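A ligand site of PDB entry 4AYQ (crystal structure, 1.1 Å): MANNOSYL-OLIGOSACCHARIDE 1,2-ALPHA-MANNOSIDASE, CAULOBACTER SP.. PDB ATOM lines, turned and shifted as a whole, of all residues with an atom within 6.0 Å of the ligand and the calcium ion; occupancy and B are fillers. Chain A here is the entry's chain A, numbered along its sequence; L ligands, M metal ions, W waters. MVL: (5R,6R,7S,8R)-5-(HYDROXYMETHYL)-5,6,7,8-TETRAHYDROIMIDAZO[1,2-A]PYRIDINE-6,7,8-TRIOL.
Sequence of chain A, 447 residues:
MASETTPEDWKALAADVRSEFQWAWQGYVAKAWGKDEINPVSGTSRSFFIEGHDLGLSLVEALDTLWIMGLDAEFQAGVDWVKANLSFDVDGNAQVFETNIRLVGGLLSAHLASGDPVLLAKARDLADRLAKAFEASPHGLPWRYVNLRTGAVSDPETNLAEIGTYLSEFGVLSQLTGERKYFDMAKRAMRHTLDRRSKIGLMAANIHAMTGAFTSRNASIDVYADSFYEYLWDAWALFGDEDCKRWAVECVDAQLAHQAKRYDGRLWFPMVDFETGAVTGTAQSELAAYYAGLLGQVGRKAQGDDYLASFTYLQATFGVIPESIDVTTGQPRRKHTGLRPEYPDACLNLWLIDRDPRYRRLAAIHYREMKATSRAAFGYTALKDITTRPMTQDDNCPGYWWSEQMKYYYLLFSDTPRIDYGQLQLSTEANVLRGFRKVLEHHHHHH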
ATOM      1  N   PHE A  97      20.695 -10.019  27.467  1.00  0.00           N
ATOM      2  CA  PHE A  97      20.586 -11.117  26.495  1.00  0.00           C
ATOM      3  C   PHE A  97      20.218 -12.417  27.196  1.00  0.00           C
ATOM      4  O   PHE A  97      19.292 -13.116  26.786  1.00  0.00           O
ATOM      5  CB  PHE A  97      21.945 -11.223  25.813  1.00  0.00           C
ATOM      6  CG  PHE A  97      22.204 -12.509  25.084  1.00  0.00           C
ATOM      7  CD1 PHE A  97      21.604 -12.793  23.875  1.00  0.00           C
ATOM      8  CD2 PHE A  97      23.137 -13.415  25.576  1.00  0.00           C
ATOM      9  CE1 PHE A  97      21.893 -13.967  23.196  1.00  0.00           C
ATOM     10  CE2 PHE A  97      23.429 -14.569  24.908  1.00  0.00           C
ATOM     11  CZ  PHE A  97      22.814 -14.848  23.712  1.00  0.00           C
ATOM     12  N   GLU A  98      20.971 -12.781  28.229  1.00  0.00           N
ATOM     13  CA  GLU A  98      20.741 -14.060  28.903  1.00  0.00           C
ATOM     14  C   GLU A  98      19.389 -14.035  29.610  1.00  0.00           C
ATOM     15  O   GLU A  98      18.672 -15.019  29.642  1.00  0.00           O
ATOM     16  CB  GLU A  98      21.835 -14.366  29.901  1.00  0.00           C
ATOM     17  CG  GLU A  98      23.211 -14.591  29.283  1.00  0.00           C
ATOM     18  CD  GLU A  98      23.396 -15.881  28.506  1.00  0.00           C
ATOM     19  OE1 GLU A  98      22.433 -16.631  28.350  1.00  0.00           O
ATOM     20  OE2 GLU A  98      24.558 -16.104  28.052  1.00  0.00           O
ATOM     21  N   ILE A 101      16.699 -14.653  26.817  1.00  0.00           N
ATOM     22  CA  ILE A 101      16.581 -15.967  26.179  1.00  0.00           C
ATOM     23  C   ILE A 101      16.271 -17.057  27.196  1.00  0.00           C
ATOM     24  O   ILE A 101      15.625 -18.053  26.854  1.00  0.00           O
ATOM     25  CB  ILE A 101      17.782 -16.333  25.290  1.00  0.00           C
ATOM     26  CG1 ILE A 101      19.080 -16.540  26.073  1.00  0.00           C
ATOM     27  CG2 ILE A 101      17.940 -15.301  24.191  1.00  0.00           C
ATOM     28  CD1 ILE A 101      20.207 -17.092  25.252  1.00  0.00           C
ATOM     29  N   ARG A 102      16.741 -16.893  28.433  1.00  0.00           N
ATOM     30  CA  ARG A 102      16.483 -17.937  29.428  1.00  0.00           C
ATOM     31  C   ARG A 102      15.221 -17.738  30.226  1.00  0.00           C
ATOM     32  O   ARG A 102      14.441 -18.691  30.376  1.00  0.00           O
ATOM     33  CB  ARG A 102      17.647 -18.061  30.385  1.00  0.00           C
ATOM     34  CG  ARG A 102      18.940 -18.393  29.673  1.00  0.00           C
ATOM     35  CD  ARG A 102      20.101 -18.370  30.616  1.00  0.00           C
ATOM     36  NE  ARG A 102      21.397 -18.453  29.993  1.00  0.00           N
ATOM     37  CZ  ARG A 102      22.205 -19.480  30.108  1.00  0.00           C
ATOM     38  NH1 ARG A 102      21.845 -20.592  30.745  1.00  0.00           N
ATOM     39  NH2 ARG A 102      23.394 -19.332  29.570  1.00  0.00           N
ATOM     40  N   THR A 165      18.858 -10.931  19.724  1.00  0.00           N
ATOM     41  CA  THR A 165      18.250 -12.191  20.150  1.00  0.00           C
ATOM     42  C   THR A 165      17.101 -11.926  21.089  1.00  0.00           C
ATOM     43  O   THR A 165      17.039 -12.419  22.220  1.00  0.00           O
ATOM     44  CB  THR A 165      19.289 -13.144  20.730  1.00  0.00           C
ATOM     45  OG1 THR A 165      20.449 -13.171  19.908  1.00  0.00           O
ATOM     46  CG2 THR A 165      18.730 -14.550  20.808  1.00  0.00           C
ATOM     47  N   ASP A 226      25.991 -15.568  16.642  1.00  0.00           N
ATOM     48  CA  ASP A 226      25.148 -16.711  16.357  1.00  0.00           C
ATOM     49  C   ASP A 226      23.646 -16.445  16.167  1.00  0.00           C
ATOM     50  O   ASP A 226      23.133 -16.517  15.046  1.00  0.00           O
ATOM     51  CB  ASP A 226      25.410 -17.849  17.372  1.00  0.00           C
ATOM     52  CG  ASP A 226      25.264 -17.493  18.857  1.00  0.00           C
ATOM     53  OD1 ASP A 226      24.886 -16.386  19.238  1.00  0.00           O
ATOM     54  OD2 ASP A 226      25.603 -18.381  19.676  1.00  0.00           O
ATOM     55  N   SER A 227      22.943 -16.191  17.258  1.00  0.00           N
ATOM     56  CA  SER A 227      21.495 -16.210  17.192  1.00  0.00           C
ATOM     57  C   SER A 227      20.873 -15.010  16.494  1.00  0.00           C
ATOM     58  O   SER A 227      19.683 -15.061  16.187  1.00  0.00           O
ATOM     59  CB  SER A 227      20.934 -16.408  18.596  1.00  0.00           C
ATOM     60  OG  SER A 227      21.534 -15.540  19.534  1.00  0.00           O
ATOM     61  N   GLU A 230      19.725 -16.627  13.352  1.00  0.00           N
ATOM     62  CA  GLU A 230      18.540 -17.449  13.592  1.00  0.00           C
ATOM     63  C   GLU A 230      17.298 -16.603  13.703  1.00  0.00           C
ATOM     64  O   GLU A 230      16.276 -16.938  13.139  1.00  0.00           O
ATOM     65  CB  GLU A 230      18.659 -18.244  14.899  1.00  0.00           C
ATOM     66  CG  GLU A 230      19.677 -19.360  14.879  1.00  0.00           C
ATOM     67  CD  GLU A 230      19.703 -20.016  16.229  1.00  0.00           C
ATOM     68  OE1 GLU A 230      20.342 -19.447  17.141  1.00  0.00           O
ATOM     69  OE2 GLU A 230      19.016 -21.075  16.399  1.00  0.00           O
ATOM     70  N   GLU A 286      32.441 -24.902  19.017  1.00  0.00           N
ATOM     71  CA  GLU A 286      31.382 -25.898  18.990  1.00  0.00           C
ATOM     72  C   GLU A 286      30.021 -25.215  18.791  1.00  0.00           C
ATOM     73  O   GLU A 286      29.116 -25.759  18.176  1.00  0.00           O
ATOM     74  CB  GLU A 286      31.372 -26.718  20.273  1.00  0.00           C
ATOM     75  CG  GLU A 286      30.356 -27.846  20.297  1.00  0.00           C
ATOM     76  CD  GLU A 286      28.945 -27.393  20.590  1.00  0.00           C
ATOM     77  OE1 GLU A 286      28.785 -26.250  21.132  1.00  0.00           O
ATOM     78  OE2 GLU A 286      28.000 -28.137  20.315  1.00  0.00           O
ATOM     79  N   LEU A 287      29.891 -24.021  19.344  1.00  0.00           N
ATOM     80  CA  LEU A 287      28.670 -23.206  19.338  1.00  0.00           C
ATOM     81  C   LEU A 287      28.164 -22.976  17.924  1.00  0.00           C
ATOM     82  O   LEU A 287      27.001 -22.723  17.710  1.00  0.00           O
ATOM     83  CB  LEU A 287      28.942 -21.832  20.043  1.00  0.00           C
ATOM     84  CG  LEU A 287      28.867 -21.753  21.577  1.00  0.00           C
ATOM     85  CD1 LEU A 287      29.489 -22.944  22.239  1.00  0.00           C
ATOM     86  CD2 LEU A 287      29.494 -20.477  22.125  1.00  0.00           C
ATOM     87  N   TYR A 290      24.938 -24.819  15.529  1.00  0.00           N
ATOM     88  CA  TYR A 290      23.563 -24.412  15.286  1.00  0.00           C
ATOM     89  C   TYR A 290      23.368 -24.053  13.808  1.00  0.00           C
ATOM     90  O   TYR A 290      22.276 -24.211  13.267  1.00  0.00           O
ATOM     91  CB  TYR A 290      23.138 -23.183  16.162  1.00  0.00           C
ATOM     92  CG  TYR A 290      23.583 -21.885  15.530  1.00  0.00           C
ATOM     93  CD1 TYR A 290      24.891 -21.444  15.647  1.00  0.00           C
ATOM     94  CD2 TYR A 290      22.738 -21.171  14.689  1.00  0.00           C
ATOM     95  CE1 TYR A 290      25.377 -20.363  14.930  1.00  0.00           C
ATOM     96  CE2 TYR A 290      23.200 -20.075  13.971  1.00  0.00           C
ATOM     97  CZ  TYR A 290      24.535 -19.686  14.091  1.00  0.00           C
ATOM     98  OH  TYR A 290      24.971 -18.624  13.328  1.00  0.00           O
ATOM     99  N   GLY A 338      31.472 -26.977  27.840  1.00  0.00           N
ATOM    100  CA  GLY A 338      30.303 -26.455  28.490  1.00  0.00           C
ATOM    101  C   GLY A 338      29.068 -27.337  28.411  1.00  0.00           C
ATOM    102  O   GLY A 338      27.964 -26.815  28.507  1.00  0.00           O
ATOM    103  N   ARG A 340      27.597 -28.799  25.894  1.00  0.00           N
ATOM    104  CA  ARG A 340      26.952 -27.942  24.910  1.00  0.00           C
ATOM    105  C   ARG A 340      25.927 -28.670  24.068  1.00  0.00           C
ATOM    106  O   ARG A 340      26.110 -29.828  23.680  1.00  0.00           O
ATOM    107  CB  ARG A 340      27.996 -27.327  24.002  1.00  0.00           C
ATOM    108  CG  ARG A 340      28.956 -26.362  24.697  1.00  0.00           C
ATOM    109  CD  ARG A 340      28.301 -25.034  25.026  1.00  0.00           C
ATOM    110  NE  ARG A 340      29.236 -24.179  25.751  1.00  0.00           N
ATOM    111  CZ  ARG A 340      28.912 -22.972  26.227  1.00  0.00           C
ATOM    112  NH1 ARG A 340      27.715 -22.468  26.032  1.00  0.00           N
ATOM    113  NH2 ARG A 340      29.828 -22.293  26.893  1.00  0.00           N
ATOM    114  N   PRO A 341      24.864 -27.947  23.673  1.00  0.00           N
ATOM    115  CA  PRO A 341      23.722 -28.551  22.992  1.00  0.00           C
ATOM    116  C   PRO A 341      23.640 -28.352  21.470  1.00  0.00           C
ATOM    117  O   PRO A 341      22.687 -28.824  20.866  1.00  0.00           O
ATOM    118  CB  PRO A 341      22.536 -27.811  23.616  1.00  0.00           C
ATOM    119  CG  PRO A 341      23.081 -26.405  23.767  1.00  0.00           C
ATOM    120  CD  PRO A 341      24.487 -26.626  24.245  1.00  0.00           C
ATOM    121  N   GLU A 342      24.602 -27.666  20.858  1.00  0.00           N
ATOM    122  CA  GLU A 342      24.371 -27.217  19.489  1.00  0.00           C
ATOM    123  C   GLU A 342      24.345 -28.321  18.442  1.00  0.00           C
ATOM    124  O   GLU A 342      23.736 -28.131  17.390  1.00  0.00           O
ATOM    125  CB  GLU A 342      25.324 -26.107  19.099  1.00  0.00           C
ATOM    126  CG  GLU A 342      25.063 -24.784  19.826  1.00  0.00           C
ATOM    127  CD  GLU A 342      25.627 -24.667  21.229  1.00  0.00           C
ATOM    128  OE1 GLU A 342      26.360 -25.579  21.690  1.00  0.00           O
ATOM    129  OE2 GLU A 342      25.308 -23.657  21.878  1.00  0.00           O
ATOM    130  N   ASP A 345      20.870 -29.735  18.462  1.00  0.00           N
ATOM    131  CA  ASP A 345      20.082 -28.605  17.917  1.00  0.00           C
ATOM    132  C   ASP A 345      20.029 -28.732  16.401  1.00  0.00           C
ATOM    133  O   ASP A 345      18.954 -28.786  15.777  1.00  0.00           O
ATOM    134  CB  ASP A 345      20.772 -27.326  18.396  1.00  0.00           C
ATOM    135  CG  ASP A 345      20.224 -26.027  17.847  1.00  0.00           C
ATOM    136  OD1 ASP A 345      19.461 -26.023  16.867  1.00  0.00           O
ATOM    137  OD2 ASP A 345      20.628 -24.988  18.399  1.00  0.00           O
ATOM    138  N   TYR A 400      21.153 -24.066  30.416  1.00  0.00           N
ATOM    139  CA  TYR A 400      20.656 -24.394  29.092  1.00  0.00           C
ATOM    140  C   TYR A 400      20.483 -25.886  28.889  1.00  0.00           C
ATOM    141  O   TYR A 400      19.698 -26.279  28.040  1.00  0.00           O
ATOM    142  CB  TYR A 400      21.495 -23.785  27.965  1.00  0.00           C
ATOM    143  CG  TYR A 400      23.009 -23.969  28.075  1.00  0.00           C
ATOM    144  CD1 TYR A 400      23.624 -25.204  27.848  1.00  0.00           C
ATOM    145  CD2 TYR A 400      23.814 -22.890  28.374  1.00  0.00           C
ATOM    146  CE1 TYR A 400      24.997 -25.336  27.938  1.00  0.00           C
ATOM    147  CE2 TYR A 400      25.187 -23.023  28.463  1.00  0.00           C
ATOM    148  CZ  TYR A 400      25.771 -24.249  28.276  1.00  0.00           C
ATOM    149  OH  TYR A 400      27.148 -24.358  28.406  1.00  0.00           O
ATOM    150  N   GLU A 404      17.572 -27.334  26.501  1.00  0.00           N
ATOM    151  CA  GLU A 404      18.050 -27.671  25.168  1.00  0.00           C
ATOM    152  C   GLU A 404      18.232 -29.166  24.909  1.00  0.00           C
ATOM    153  O   GLU A 404      17.364 -29.772  24.312  1.00  0.00           O
ATOM    154  CB  GLU A 404      19.301 -26.874  24.825  1.00  0.00           C
ATOM    155  CG  GLU A 404      19.058 -25.371  24.802  1.00  0.00           C
ATOM    156  CD  GLU A 404      20.012 -24.644  23.890  1.00  0.00           C
ATOM    157  OE1 GLU A 404      20.204 -25.071  22.740  1.00  0.00           O
ATOM    158  OE2 GLU A 404      20.578 -23.631  24.353  1.00  0.00           O
ATOM    159  N   TYR A 408      15.900 -31.678  22.799  1.00  0.00           N
ATOM    160  CA  TYR A 408      16.203 -32.067  21.418  1.00  0.00           C
ATOM    161  C   TYR A 408      16.156 -33.578  21.238  1.00  0.00           C
ATOM    162  O   TYR A 408      15.560 -34.092  20.291  1.00  0.00           O
ATOM    163  CB  TYR A 408      17.556 -31.537  20.955  1.00  0.00           C
ATOM    164  CG  TYR A 408      17.752 -30.040  20.982  1.00  0.00           C
ATOM    165  CD1 TYR A 408      16.750 -29.150  20.679  1.00  0.00           C
ATOM    166  CD2 TYR A 408      18.984 -29.499  21.312  1.00  0.00           C
ATOM    167  CE1 TYR A 408      16.950 -27.771  20.695  1.00  0.00           C
ATOM    168  CE2 TYR A 408      19.206 -28.136  21.343  1.00  0.00           C
ATOM    169  CZ  TYR A 408      18.187 -27.275  21.049  1.00  0.00           C
ATOM    170  OH  TYR A 408      18.361 -25.923  21.093  1.00  0.00           O
ATOM    171  N   SER A 427      13.043 -21.363  20.196  1.00  0.00           N
ATOM    172  CA  SER A 427      13.936 -20.231  20.357  1.00  0.00           C
ATOM    173  C   SER A 427      15.383 -20.735  20.336  1.00  0.00           C
ATOM    174  O   SER A 427      15.639 -21.933  20.285  1.00  0.00           O
ATOM    175  CB  SER A 427      13.649 -19.505  21.668  1.00  0.00           C
ATOM    176  OG  SER A 427      14.304 -20.168  22.756  1.00  0.00           O
ATOM    177  N   THR A 428      16.342 -19.816  20.438  1.00  0.00           N
ATOM    178  CA  THR A 428      17.740 -20.237  20.437  1.00  0.00           C
ATOM    179  C   THR A 428      18.143 -20.956  21.732  1.00  0.00           C
ATOM    180  O   THR A 428      19.207 -21.560  21.776  1.00  0.00           O
ATOM    181  CB  THR A 428      18.686 -19.043  20.159  1.00  0.00           C
ATOM    182  OG1 THR A 428      19.956 -19.551  19.750  1.00  0.00           O
ATOM    183  CG2 THR A 428      18.855 -18.142  21.363  1.00  0.00           C
ATOM    184  N   GLU A 429      17.292 -20.861  22.755  1.00  0.00           N
ATOM    185  CA  GLU A 429      17.418 -21.566  24.018  1.00  0.00           C
ATOM    186  C   GLU A 429      16.487 -22.784  24.062  1.00  0.00           C
ATOM    187  O   GLU A 429      16.258 -23.373  25.110  1.00  0.00           O
ATOM    188  CB  GLU A 429      17.083 -20.578  25.145  1.00  0.00           C
ATOM    189  CG  GLU A 429      17.440 -21.003  26.551  1.00  0.00           C
ATOM    190  CD  GLU A 429      18.913 -20.971  26.897  1.00  0.00           C
ATOM    191  OE1 GLU A 429      19.717 -20.414  26.119  1.00  0.00           O
ATOM    192  OE2 GLU A 429      19.291 -21.475  27.990  1.00  0.00           O
HETATM  193  C1  MVL L   1      23.964 -19.851  23.090  1.00  0.00           C
HETATM  194  N10 MVL L   1      24.649 -20.640  23.939  1.00  0.00           N
HETATM  195  C3  MVL L   1      21.824 -20.792  23.822  1.00  0.00           C
HETATM  196  C4  MVL L   1      22.529 -21.139  25.146  1.00  0.00           C
HETATM  197  C5  MVL L   1      24.010 -21.476  24.989  1.00  0.00           C
HETATM  198  C6  MVL L   1      24.177 -22.963  24.635  1.00  0.00           C
HETATM  199  C7  MVL L   1      26.115 -19.716  22.592  1.00  0.00           C
HETATM  200  C8  MVL L   1      25.973 -20.546  23.644  1.00  0.00           C
HETATM  201  N1  MVL L   1      24.864 -19.303  22.267  1.00  0.00           N
HETATM  202  O3  MVL L   1      21.843 -21.901  22.933  1.00  0.00           O
HETATM  203  O2  MVL L   1      21.939 -19.475  21.835  1.00  0.00           O
HETATM  204  O4  MVL L   1      22.422 -20.025  26.030  1.00  0.00           O
HETATM  205  C2  MVL L   1      22.505 -19.629  23.132  1.00  0.00           C
HETATM  206  O6  MVL L   1      25.545 -23.324  24.458  1.00  0.00           O
HETATM  207 CA    CA M   1      21.355 -21.486  20.552  1.00  0.00          CA
HETATM  208  O   HOH W   1      22.506 -20.326  18.681  1.00  0.00           O
HETATM  209  O   HOH W   2      24.559 -18.156  26.214  1.00  0.00           O
HETATM  210  O   HOH W   3      20.120 -22.337  18.662  1.00  0.00           O
HETATM  211  O   HOH W   4      26.203 -16.825  24.261  1.00  0.00           O
HETATM  212  O   HOH W   5      22.911 -17.080  21.210  1.00  0.00           O
HETATM  213  O   HOH W   6      23.717 -21.805  20.702  1.00  0.00           O
HETATM  214  O   HOH W   7      21.541 -23.885  20.756  1.00  0.00           O
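Ile 101 touches the ligand (CD1 to O4, 3.8 Å).
NH2 of Arg 102 touches O4 of the ligand, 3.7 Å away.
CD2 of Leu 287 touches C7 of the ligand (3.5 Å).
Pro 341 touches the ligand.
Tyr 400 touches the ligand.
Hydrophobic or aromatic side chains that line the ligand: Ile 101, Leu 287, Pro 341 and Tyr 400.
11 residues have an atom within 4 Å of the ligand: Ile 101, Arg 102, Asp 226, Leu 287, Arg 340, Pro 341, Glu 342, Tyr 400, Glu 404, Thr 428 and Glu 429.
The nearest printed residue that does not touch the ligand is Glu 98 (4.1 Å).
Within 4 Å of the calcium ion: Thr 428.
The nearest printed residue that does not touch the calcium ion is Glu 230 (4.1 Å).
Water W6 bridges OE2 of Glu 342 and N1 of the ligand.
Water W7 lies within hydrogen-bond range of OE1 of Glu 404 (2.7 Å) and OD2 of Asp 345 (2.8 Å).
Water W3 bridges the side-chain carboxylate (OD2) of Asp 345 and the side-chain carboxylate (OE1) of Glu 230.
Water W5 lies within hydrogen-bond range of the side-chain hydroxyl (OG) of Ser 227 (2.7 Å), the side-chain carboxylate (OD1) of Asp 226 (2.9 Å) and a nitrogen (N1) of the ligand (3.1 Å).
Water W2 lies within hydrogen-bond range of OE2 of Glu 98 (2.8 Å) and O4 of the ligand (2.8 Å).
OE1 of Glu 98 lies within salt-bridge range of NE of Arg 102.
The backbone NH of Glu 429 lies within hydrogen-bond range of the side-chain hydroxyl of Ser 427 (3.1 Å).
OE1 of Glu 404 sits at hydrogen-bond distance from OH of Tyr 408.
OG of Ser 227 sits at hydrogen-bond distance from OD1 of Asp 226, 3.5 Å away.
N of Glu 342 sits at hydrogen-bond distance from OE2 of Glu 286, 3.5 Å away.
OE2 of Glu 429 lies within salt-bridge range of NH1 of Arg 102, 3.9 Å away.
The side-chain hydroxyl (OG1) of Thr 428 lies close to the side-chain carboxylate (OE1) of Glu 230, 2.6 Å away.
The backbone carbonyl oxygen (O) of Gly 338 is in hydrogen-bond range of the side-chain hydroxyl (OH) of Tyr 400 (2.6 Å).
The calcium ion is bound by water W6.
The calcium ion is bound by water W3 (2.4 Å).
Water W7 is bound to the calcium ion, at 2.4 Å.
O2 of the ligand is bound to the calcium ion.
O3 of the ligand is bound to the calcium ion (2.5 Å).
The calcium ion is bound by O of Thr 428 (2.5 Å).
Water W1 is bound to the calcium ion.
The calcium ion is bound by OG1 of Thr 428.
An oxygen (O4) of the ligand lies within hydrogen-bond range of the side-chain carboxylate of Glu 429 (2.7 Å).
OE2 of Glu 342 sits at hydrogen-bond distance from O6 of the ligand.
The side-chain carboxylate of Asp 226 sits at hydrogen-bond distance from a nitrogen (N1) of the ligand (2.8 Å).
The guanidinium group (NH1) of Arg 340 lies within hydrogen-bond range of an oxygen (O6) of the ligand.
The side-chain carboxylate of Glu 404 lies close to an oxygen (O3) of the ligand (2.6 Å).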
